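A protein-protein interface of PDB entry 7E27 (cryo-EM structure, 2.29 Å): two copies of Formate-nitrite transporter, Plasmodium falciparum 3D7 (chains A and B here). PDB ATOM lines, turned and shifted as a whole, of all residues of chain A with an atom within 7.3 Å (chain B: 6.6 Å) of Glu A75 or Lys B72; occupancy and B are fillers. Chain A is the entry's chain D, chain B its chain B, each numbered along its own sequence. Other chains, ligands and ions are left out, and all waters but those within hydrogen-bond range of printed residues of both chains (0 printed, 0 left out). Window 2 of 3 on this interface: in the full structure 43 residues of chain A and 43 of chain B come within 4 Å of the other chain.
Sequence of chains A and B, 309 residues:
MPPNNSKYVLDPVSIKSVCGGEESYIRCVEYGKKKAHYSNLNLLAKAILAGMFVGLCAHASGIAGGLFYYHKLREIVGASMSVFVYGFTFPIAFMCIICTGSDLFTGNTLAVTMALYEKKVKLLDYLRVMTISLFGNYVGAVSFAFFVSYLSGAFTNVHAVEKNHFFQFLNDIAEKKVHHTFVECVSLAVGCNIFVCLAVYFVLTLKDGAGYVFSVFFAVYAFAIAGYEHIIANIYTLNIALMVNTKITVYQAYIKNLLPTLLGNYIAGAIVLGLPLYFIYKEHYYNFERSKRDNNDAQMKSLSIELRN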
ATOM      1  N   TYR A  69      19.938   4.632 -25.422  1.00  0.00           N
ATOM      2  CA  TYR A  69      19.076   3.471 -25.559  1.00  0.00           C
ATOM      3  C   TYR A  69      19.083   2.921 -26.976  1.00  0.00           C
ATOM      4  O   TYR A  69      18.129   2.247 -27.374  1.00  0.00           O
ATOM      5  CB  TYR A  69      17.653   3.830 -25.140  1.00  0.00           C
ATOM      6  CG  TYR A  69      16.864   2.702 -24.533  1.00  0.00           C
ATOM      7  CD1 TYR A  69      17.311   2.051 -23.392  1.00  0.00           C
ATOM      8  CD2 TYR A  69      15.663   2.296 -25.095  1.00  0.00           C
ATOM      9  CE1 TYR A  69      16.583   1.026 -22.832  1.00  0.00           C
ATOM     10  CE2 TYR A  69      14.931   1.278 -24.543  1.00  0.00           C
ATOM     11  CZ  TYR A  69      15.391   0.646 -23.414  1.00  0.00           C
ATOM     12  OH  TYR A  69      14.656  -0.373 -22.869  1.00  0.00           O
ATOM     13  N   TYR A  70      20.119   3.240 -27.749  1.00  0.00           N
ATOM     14  CA  TYR A  70      20.309   2.694 -29.084  1.00  0.00           C
ATOM     15  C   TYR A  70      20.420   1.177 -29.010  1.00  0.00           C
ATOM     16  O   TYR A  70      21.014   0.631 -28.079  1.00  0.00           O
ATOM     17  CB  TYR A  70      21.564   3.306 -29.706  1.00  0.00           C
ATOM     18  CG  TYR A  70      21.821   2.936 -31.142  1.00  0.00           C
ATOM     19  CD1 TYR A  70      21.080   3.502 -32.168  1.00  0.00           C
ATOM     20  CD2 TYR A  70      22.821   2.031 -31.472  1.00  0.00           C
ATOM     21  CE1 TYR A  70      21.318   3.166 -33.481  1.00  0.00           C
ATOM     22  CE2 TYR A  70      23.065   1.692 -32.777  1.00  0.00           C
ATOM     23  CZ  TYR A  70      22.312   2.261 -33.777  1.00  0.00           C
ATOM     24  OH  TYR A  70      22.559   1.920 -35.081  1.00  0.00           O
ATOM     25  N   HIS A  71      19.834   0.499 -30.002  1.00  0.00           N
ATOM     26  CA  HIS A  71      19.512  -0.920 -29.855  1.00  0.00           C
ATOM     27  C   HIS A  71      20.761  -1.798 -29.818  1.00  0.00           C
ATOM     28  O   HIS A  71      20.807  -2.779 -29.067  1.00  0.00           O
ATOM     29  CB  HIS A  71      18.545  -1.359 -30.960  1.00  0.00           C
ATOM     30  CG  HIS A  71      19.118  -1.328 -32.344  1.00  0.00           C
ATOM     31  ND1 HIS A  71      19.072  -2.418 -33.184  1.00  0.00           N
ATOM     32  CD2 HIS A  71      19.723  -0.341 -33.045  1.00  0.00           C
ATOM     33  CE1 HIS A  71      19.631  -2.107 -34.338  1.00  0.00           C
ATOM     34  NE2 HIS A  71      20.040  -0.854 -34.277  1.00  0.00           N
ATOM     35  N   LYS A  72      21.806  -1.428 -30.560  1.00  0.00           N
ATOM     36  CA  LYS A  72      23.053  -2.186 -30.506  1.00  0.00           C
ATOM     37  C   LYS A  72      23.782  -1.970 -29.185  1.00  0.00           C
ATOM     38  O   LYS A  72      24.445  -2.882 -28.682  1.00  0.00           O
ATOM     39  CB  LYS A  72      23.950  -1.812 -31.682  1.00  0.00           C
ATOM     40  CG  LYS A  72      23.280  -1.917 -33.030  1.00  0.00           C
ATOM     41  CD  LYS A  72      22.768  -3.311 -33.284  1.00  0.00           C
ATOM     42  CE  LYS A  72      23.893  -4.270 -33.562  1.00  0.00           C
ATOM     43  NZ  LYS A  72      23.384  -5.645 -33.786  1.00  0.00           N
ATOM     44  N   LEU A  73      23.677  -0.771 -28.611  1.00  0.00           N
ATOM     45  CA  LEU A  73      24.228  -0.535 -27.281  1.00  0.00           C
ATOM     46  C   LEU A  73      23.347  -1.166 -26.210  1.00  0.00           C
ATOM     47  O   LEU A  73      23.842  -1.622 -25.172  1.00  0.00           O
ATOM     48  CB  LEU A  73      24.386   0.968 -27.046  1.00  0.00           C
ATOM     49  CG  LEU A  73      25.009   1.435 -25.732  1.00  0.00           C
ATOM     50  CD1 LEU A  73      26.428   0.918 -25.609  1.00  0.00           C
ATOM     51  CD2 LEU A  73      24.973   2.944 -25.639  1.00  0.00           C
ATOM     52  N   ARG A  74      22.037  -1.211 -26.462  1.00  0.00           N
ATOM     53  CA  ARG A  74      21.089  -1.791 -25.517  1.00  0.00           C
ATOM     54  C   ARG A  74      21.255  -3.302 -25.413  1.00  0.00           C
ATOM     55  O   ARG A  74      20.943  -3.895 -24.375  1.00  0.00           O
ATOM     56  CB  ARG A  74      19.669  -1.425 -25.950  1.00  0.00           C
ATOM     57  CG  ARG A  74      18.582  -1.609 -24.927  1.00  0.00           C
ATOM     58  CD  ARG A  74      17.240  -1.686 -25.624  1.00  0.00           C
ATOM     59  NE  ARG A  74      17.094  -0.623 -26.611  1.00  0.00           N
ATOM     60  CZ  ARG A  74      16.238  -0.649 -27.628  1.00  0.00           C
ATOM     61  NH1 ARG A  74      16.182   0.370 -28.471  1.00  0.00           N
ATOM     62  NH2 ARG A  74      15.441  -1.690 -27.802  1.00  0.00           N
ATOM     63  N   GLU A  75      21.745  -3.946 -26.478  1.00  0.00           N
ATOM     64  CA  GLU A  75      22.035  -5.376 -26.395  1.00  0.00           C
ATOM     65  C   GLU A  75      23.234  -5.665 -25.495  1.00  0.00           C
ATOM     66  O   GLU A  75      23.352  -6.764 -24.946  1.00  0.00           O
ATOM     67  CB  GLU A  75      22.280  -5.960 -27.784  1.00  0.00           C
ATOM     68  CG  GLU A  75      21.067  -5.965 -28.688  1.00  0.00           C
ATOM     69  CD  GLU A  75      21.386  -6.445 -30.086  1.00  0.00           C
ATOM     70  OE1 GLU A  75      22.549  -6.291 -30.506  1.00  0.00           O
ATOM     71  OE2 GLU A  75      20.469  -6.949 -30.768  1.00  0.00           O
ATOM     72  N   ILE A  76      24.145  -4.703 -25.349  1.00  0.00           N
ATOM     73  CA  ILE A  76      25.348  -4.957 -24.563  1.00  0.00           C
ATOM     74  C   ILE A  76      25.159  -4.512 -23.119  1.00  0.00           C
ATOM     75  O   ILE A  76      25.423  -5.276 -22.186  1.00  0.00           O
ATOM     76  CB  ILE A  76      26.571  -4.280 -25.207  1.00  0.00           C
ATOM     77  CG1 ILE A  76      26.764  -4.770 -26.642  1.00  0.00           C
ATOM     78  CG2 ILE A  76      27.822  -4.547 -24.386  1.00  0.00           C
ATOM     79  CD1 ILE A  76      27.632  -3.866 -27.477  1.00  0.00           C
ATOM     80  N   VAL A  77      24.710  -3.277 -22.899  1.00  0.00           N
ATOM     81  CA  VAL A  77      24.699  -2.709 -21.554  1.00  0.00           C
ATOM     82  C   VAL A  77      23.316  -2.684 -20.934  1.00  0.00           C
ATOM     83  O   VAL A  77      23.192  -2.345 -19.750  1.00  0.00           O
ATOM     84  CB  VAL A  77      25.320  -1.299 -21.528  1.00  0.00           C
ATOM     85  CG1 VAL A  77      26.691  -1.308 -22.167  1.00  0.00           C
ATOM     86  CG2 VAL A  77      24.409  -0.286 -22.192  1.00  0.00           C
ATOM     87  N   GLY A  78      22.275  -3.042 -21.679  1.00  0.00           N
ATOM     88  CA  GLY A  78      20.936  -2.935 -21.136  1.00  0.00           C
ATOM     89  C   GLY A  78      20.484  -1.492 -21.064  1.00  0.00           C
ATOM     90  O   GLY A  78      20.663  -0.709 -22.001  1.00  0.00           O
ATOM     91  N   TYR B  69      25.503  -4.101 -13.572  1.00  0.00           N
ATOM     92  CA  TYR B  69      25.754  -5.521 -13.394  1.00  0.00           C
ATOM     93  C   TYR B  69      24.952  -6.367 -14.371  1.00  0.00           C
ATOM     94  O   TYR B  69      24.708  -7.545 -14.101  1.00  0.00           O
ATOM     95  CB  TYR B  69      25.434  -5.929 -11.959  1.00  0.00           C
ATOM     96  CG  TYR B  69      26.269  -7.057 -11.417  1.00  0.00           C
ATOM     97  CD1 TYR B  69      27.652  -6.955 -11.353  1.00  0.00           C
ATOM     98  CD2 TYR B  69      25.673  -8.221 -10.956  1.00  0.00           C
ATOM     99  CE1 TYR B  69      28.414  -7.983 -10.847  1.00  0.00           C
ATOM    100  CE2 TYR B  69      26.423  -9.248 -10.449  1.00  0.00           C
ATOM    101  CZ  TYR B  69      27.791  -9.127 -10.395  1.00  0.00           C
ATOM    102  OH  TYR B  69      28.536 -10.160  -9.891  1.00  0.00           O
ATOM    103  N   TYR B  70      24.507  -5.767 -15.473  1.00  0.00           N
ATOM    104  CA  TYR B  70      23.826  -6.481 -16.543  1.00  0.00           C
ATOM    105  C   TYR B  70      24.742  -7.555 -17.113  1.00  0.00           C
ATOM    106  O   TYR B  70      25.950  -7.353 -17.239  1.00  0.00           O
ATOM    107  CB  TYR B  70      23.406  -5.488 -17.626  1.00  0.00           C
ATOM    108  CG  TYR B  70      22.573  -6.059 -18.741  1.00  0.00           C
ATOM    109  CD1 TYR B  70      21.234  -6.358 -18.548  1.00  0.00           C
ATOM    110  CD2 TYR B  70      23.123  -6.282 -19.995  1.00  0.00           C
ATOM    111  CE1 TYR B  70      20.470  -6.877 -19.569  1.00  0.00           C
ATOM    112  CE2 TYR B  70      22.370  -6.796 -21.017  1.00  0.00           C
ATOM    113  CZ  TYR B  70      21.046  -7.093 -20.800  1.00  0.00           C
ATOM    114  OH  TYR B  70      20.296  -7.608 -21.825  1.00  0.00           O
ATOM    115  N   HIS B  71      24.155  -8.706 -17.449  1.00  0.00           N
ATOM    116  CA  HIS B  71      24.938  -9.930 -17.616  1.00  0.00           C
ATOM    117  C   HIS B  71      25.839  -9.881 -18.847  1.00  0.00           C
ATOM    118  O   HIS B  71      26.970 -10.377 -18.809  1.00  0.00           O
ATOM    119  CB  HIS B  71      24.011 -11.151 -17.643  1.00  0.00           C
ATOM    120  CG  HIS B  71      23.099 -11.221 -18.829  1.00  0.00           C
ATOM    121  ND1 HIS B  71      23.024 -12.335 -19.635  1.00  0.00           N
ATOM    122  CD2 HIS B  71      22.210 -10.334 -19.334  1.00  0.00           C
ATOM    123  CE1 HIS B  71      22.136 -12.128 -20.588  1.00  0.00           C
ATOM    124  NE2 HIS B  71      21.631 -10.919 -20.431  1.00  0.00           N
ATOM    125  N   LYS B  72      25.392  -9.226 -19.921  1.00  0.00           N
ATOM    126  CA  LYS B  72      26.240  -9.082 -21.100  1.00  0.00           C
ATOM    127  C   LYS B  72      27.380  -8.101 -20.851  1.00  0.00           C
ATOM    128  O   LYS B  72      28.477  -8.269 -21.393  1.00  0.00           O
ATOM    129  CB  LYS B  72      25.407  -8.640 -22.300  1.00  0.00           C
ATOM    130  CG  LYS B  72      24.204  -9.512 -22.571  1.00  0.00           C
ATOM    131  CD  LYS B  72      24.601 -10.945 -22.806  1.00  0.00           C
ATOM    132  CE  LYS B  72      25.263 -11.122 -24.145  1.00  0.00           C
ATOM    133  NZ  LYS B  72      25.675 -12.531 -24.358  1.00  0.00           N
ATOM    134  N   LEU B  73      27.142  -7.070 -20.039  1.00  0.00           N
ATOM    135  CA  LEU B  73      28.222  -6.175 -19.643  1.00  0.00           C
ATOM    136  C   LEU B  73      29.119  -6.833 -18.603  1.00  0.00           C
ATOM    137  O   LEU B  73      30.330  -6.587 -18.564  1.00  0.00           O
ATOM    138  CB  LEU B  73      27.639  -4.864 -19.112  1.00  0.00           C
ATOM    139  CG  LEU B  73      28.603  -3.754 -18.700  1.00  0.00           C
ATOM    140  CD1 LEU B  73      29.429  -3.305 -19.889  1.00  0.00           C
ATOM    141  CD2 LEU B  73      27.844  -2.592 -18.098  1.00  0.00           C
ATOM    142  N   ARG B  74      28.534  -7.690 -17.764  1.00  0.00           N
ATOM    143  CA  ARG B  74      29.283  -8.386 -16.723  1.00  0.00           C
ATOM    144  C   ARG B  74      30.237  -9.416 -17.316  1.00  0.00           C
ATOM    145  O   ARG B  74      31.268  -9.733 -16.712  1.00  0.00           O
ATOM    146  CB  ARG B  74      28.298  -9.045 -15.757  1.00  0.00           C
ATOM    147  CG  ARG B  74      28.849  -9.495 -14.432  1.00  0.00           C
ATOM    148  CD  ARG B  74      27.925 -10.528 -13.824  1.00  0.00           C
ATOM    149  NE  ARG B  74      26.534 -10.098 -13.889  1.00  0.00           N
ATOM    150  CZ  ARG B  74      25.486 -10.912 -13.808  1.00  0.00           C
ATOM    151  NH1 ARG B  74      24.259 -10.420 -13.878  1.00  0.00           N
ATOM    152  NH2 ARG B  74      25.664 -12.214 -13.661  1.00  0.00           N
ATOM    153  N   GLU B  75      29.915  -9.952 -18.497  1.00  0.00           N
ATOM    154  CA  GLU B  75      30.848 -10.855 -19.167  1.00  0.00           C
ATOM    155  C   GLU B  75      32.083 -10.121 -19.681  1.00  0.00           C
ATOM    156  O   GLU B  75      33.146 -10.728 -19.850  1.00  0.00           O
ATOM    157  CB  GLU B  75      30.164 -11.583 -20.322  1.00  0.00           C
ATOM    158  CG  GLU B  75      29.079 -12.551 -19.901  1.00  0.00           C
ATOM    159  CD  GLU B  75      28.354 -13.160 -21.080  1.00  0.00           C
ATOM    160  OE1 GLU B  75      28.311 -12.506 -22.141  1.00  0.00           O
ATOM    161  OE2 GLU B  75      27.807 -14.273 -20.934  1.00  0.00           O
ATOM    162  N   ILE B  76      31.963  -8.823 -19.959  1.00  0.00           N
ATOM    163  CA  ILE B  76      33.093  -8.096 -20.527  1.00  0.00           C
ATOM    164  C   ILE B  76      33.915  -7.424 -19.433  1.00  0.00           C
ATOM    165  O   ILE B  76      35.138  -7.577 -19.384  1.00  0.00           O
ATOM    166  CB  ILE B  76      32.611  -7.076 -21.575  1.00  0.00           C
ATOM    167  CG1 ILE B  76      31.824  -7.776 -22.682  1.00  0.00           C
ATOM    168  CG2 ILE B  76      33.792  -6.321 -22.166  1.00  0.00           C
ATOM    169  CD1 ILE B  76      30.959  -6.843 -23.488  1.00  0.00           C
ATOM    170  N   VAL B  77      33.273  -6.669 -18.544  1.00  0.00           N
ATOM    171  CA  VAL B  77      34.006  -5.834 -17.598  1.00  0.00           C
ATOM    172  C   VAL B  77      34.036  -6.414 -16.197  1.00  0.00           C
ATOM    173  O   VAL B  77      34.733  -5.867 -15.332  1.00  0.00           O
ATOM    174  CB  VAL B  77      33.457  -4.394 -17.566  1.00  0.00           C
ATOM    175  CG1 VAL B  77      33.398  -3.815 -18.962  1.00  0.00           C
ATOM    176  CG2 VAL B  77      32.101  -4.340 -16.888  1.00  0.00           C
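N of Leu B73 lies within hydrogen-bond range of O of Ile A76 (3.3 Å).
The side-chain carboxylate (OE1) of Glu A75 lies within salt-bridge range of the side-chain amino group (NZ) of Lys A72, at 3.4 Å. NZ of Lys B72 is in salt-bridge range of OE1 of Glu B75, at 3.4 Å.
O of Glu A75 touches CG of Lys B72, 3.7 Å away. Ile A76 touches Tyr B70. O of Ile A76 touches CB of Lys B72 (3.4 Å). Ile A76 touches Ile B76. Tyr B70 touches Val A77. CD2 of Tyr B70 touches N of Gly A78, at 3.7 Å.
Lys B72 touches just these residues of chain A: Glu A75 (3.7 Å) and Ile A76 (3.4 Å). Of the printed residues of chain A, Ile B76 touches Ile A76. Of the printed residues of chain A, Leu B73 touches Ile A76. The nearest printed residue of chain A that does not touch Ile B76 is Val A77 (7.1 Å).
Printed residues of chain B that touch a printed residue of chain A: Tyr B70, Lys B72, Leu B73 and Ile B76. Of the 10 printed residues of chain A, 4 touch a printed residue of chain B. Printed residues of chain A that touch a printed residue of chain B: Glu A75, Ile A76, Val A77 and Gly A78. Hydrophobic or aromatic side chains of chain A that line the printed part of chain B: Ile A76. Along chain A the printed residues that touch a printed residue of chain B span positions 75 to 78. Among the printed residues, no Asp or Glu carboxylate lies within 4 Å of a Lys or Arg side-chain nitrogen of the other chain.
Glu A75 touches Lys B72, but with the chains exchanged Lys A72 does not touch Glu B75 (12.3 Å). Ile A76 touches Leu B73, but with the chains exchanged Leu A73 does not touch Ile B76 (9.0 Å). Ile B76 touches its own counterpart, Ile A76. Val A77 touches Tyr B70, but with the chains exchanged Tyr A70 does not touch Val B77 (16.0 Å). Positions printed for both chains: 69, 70, 71, 72, 73, 74, 75, 76 and 77. Of the 7 pairs that touch across the chains among the printed residues, 1 has its exchanged pair printed and touching as well.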
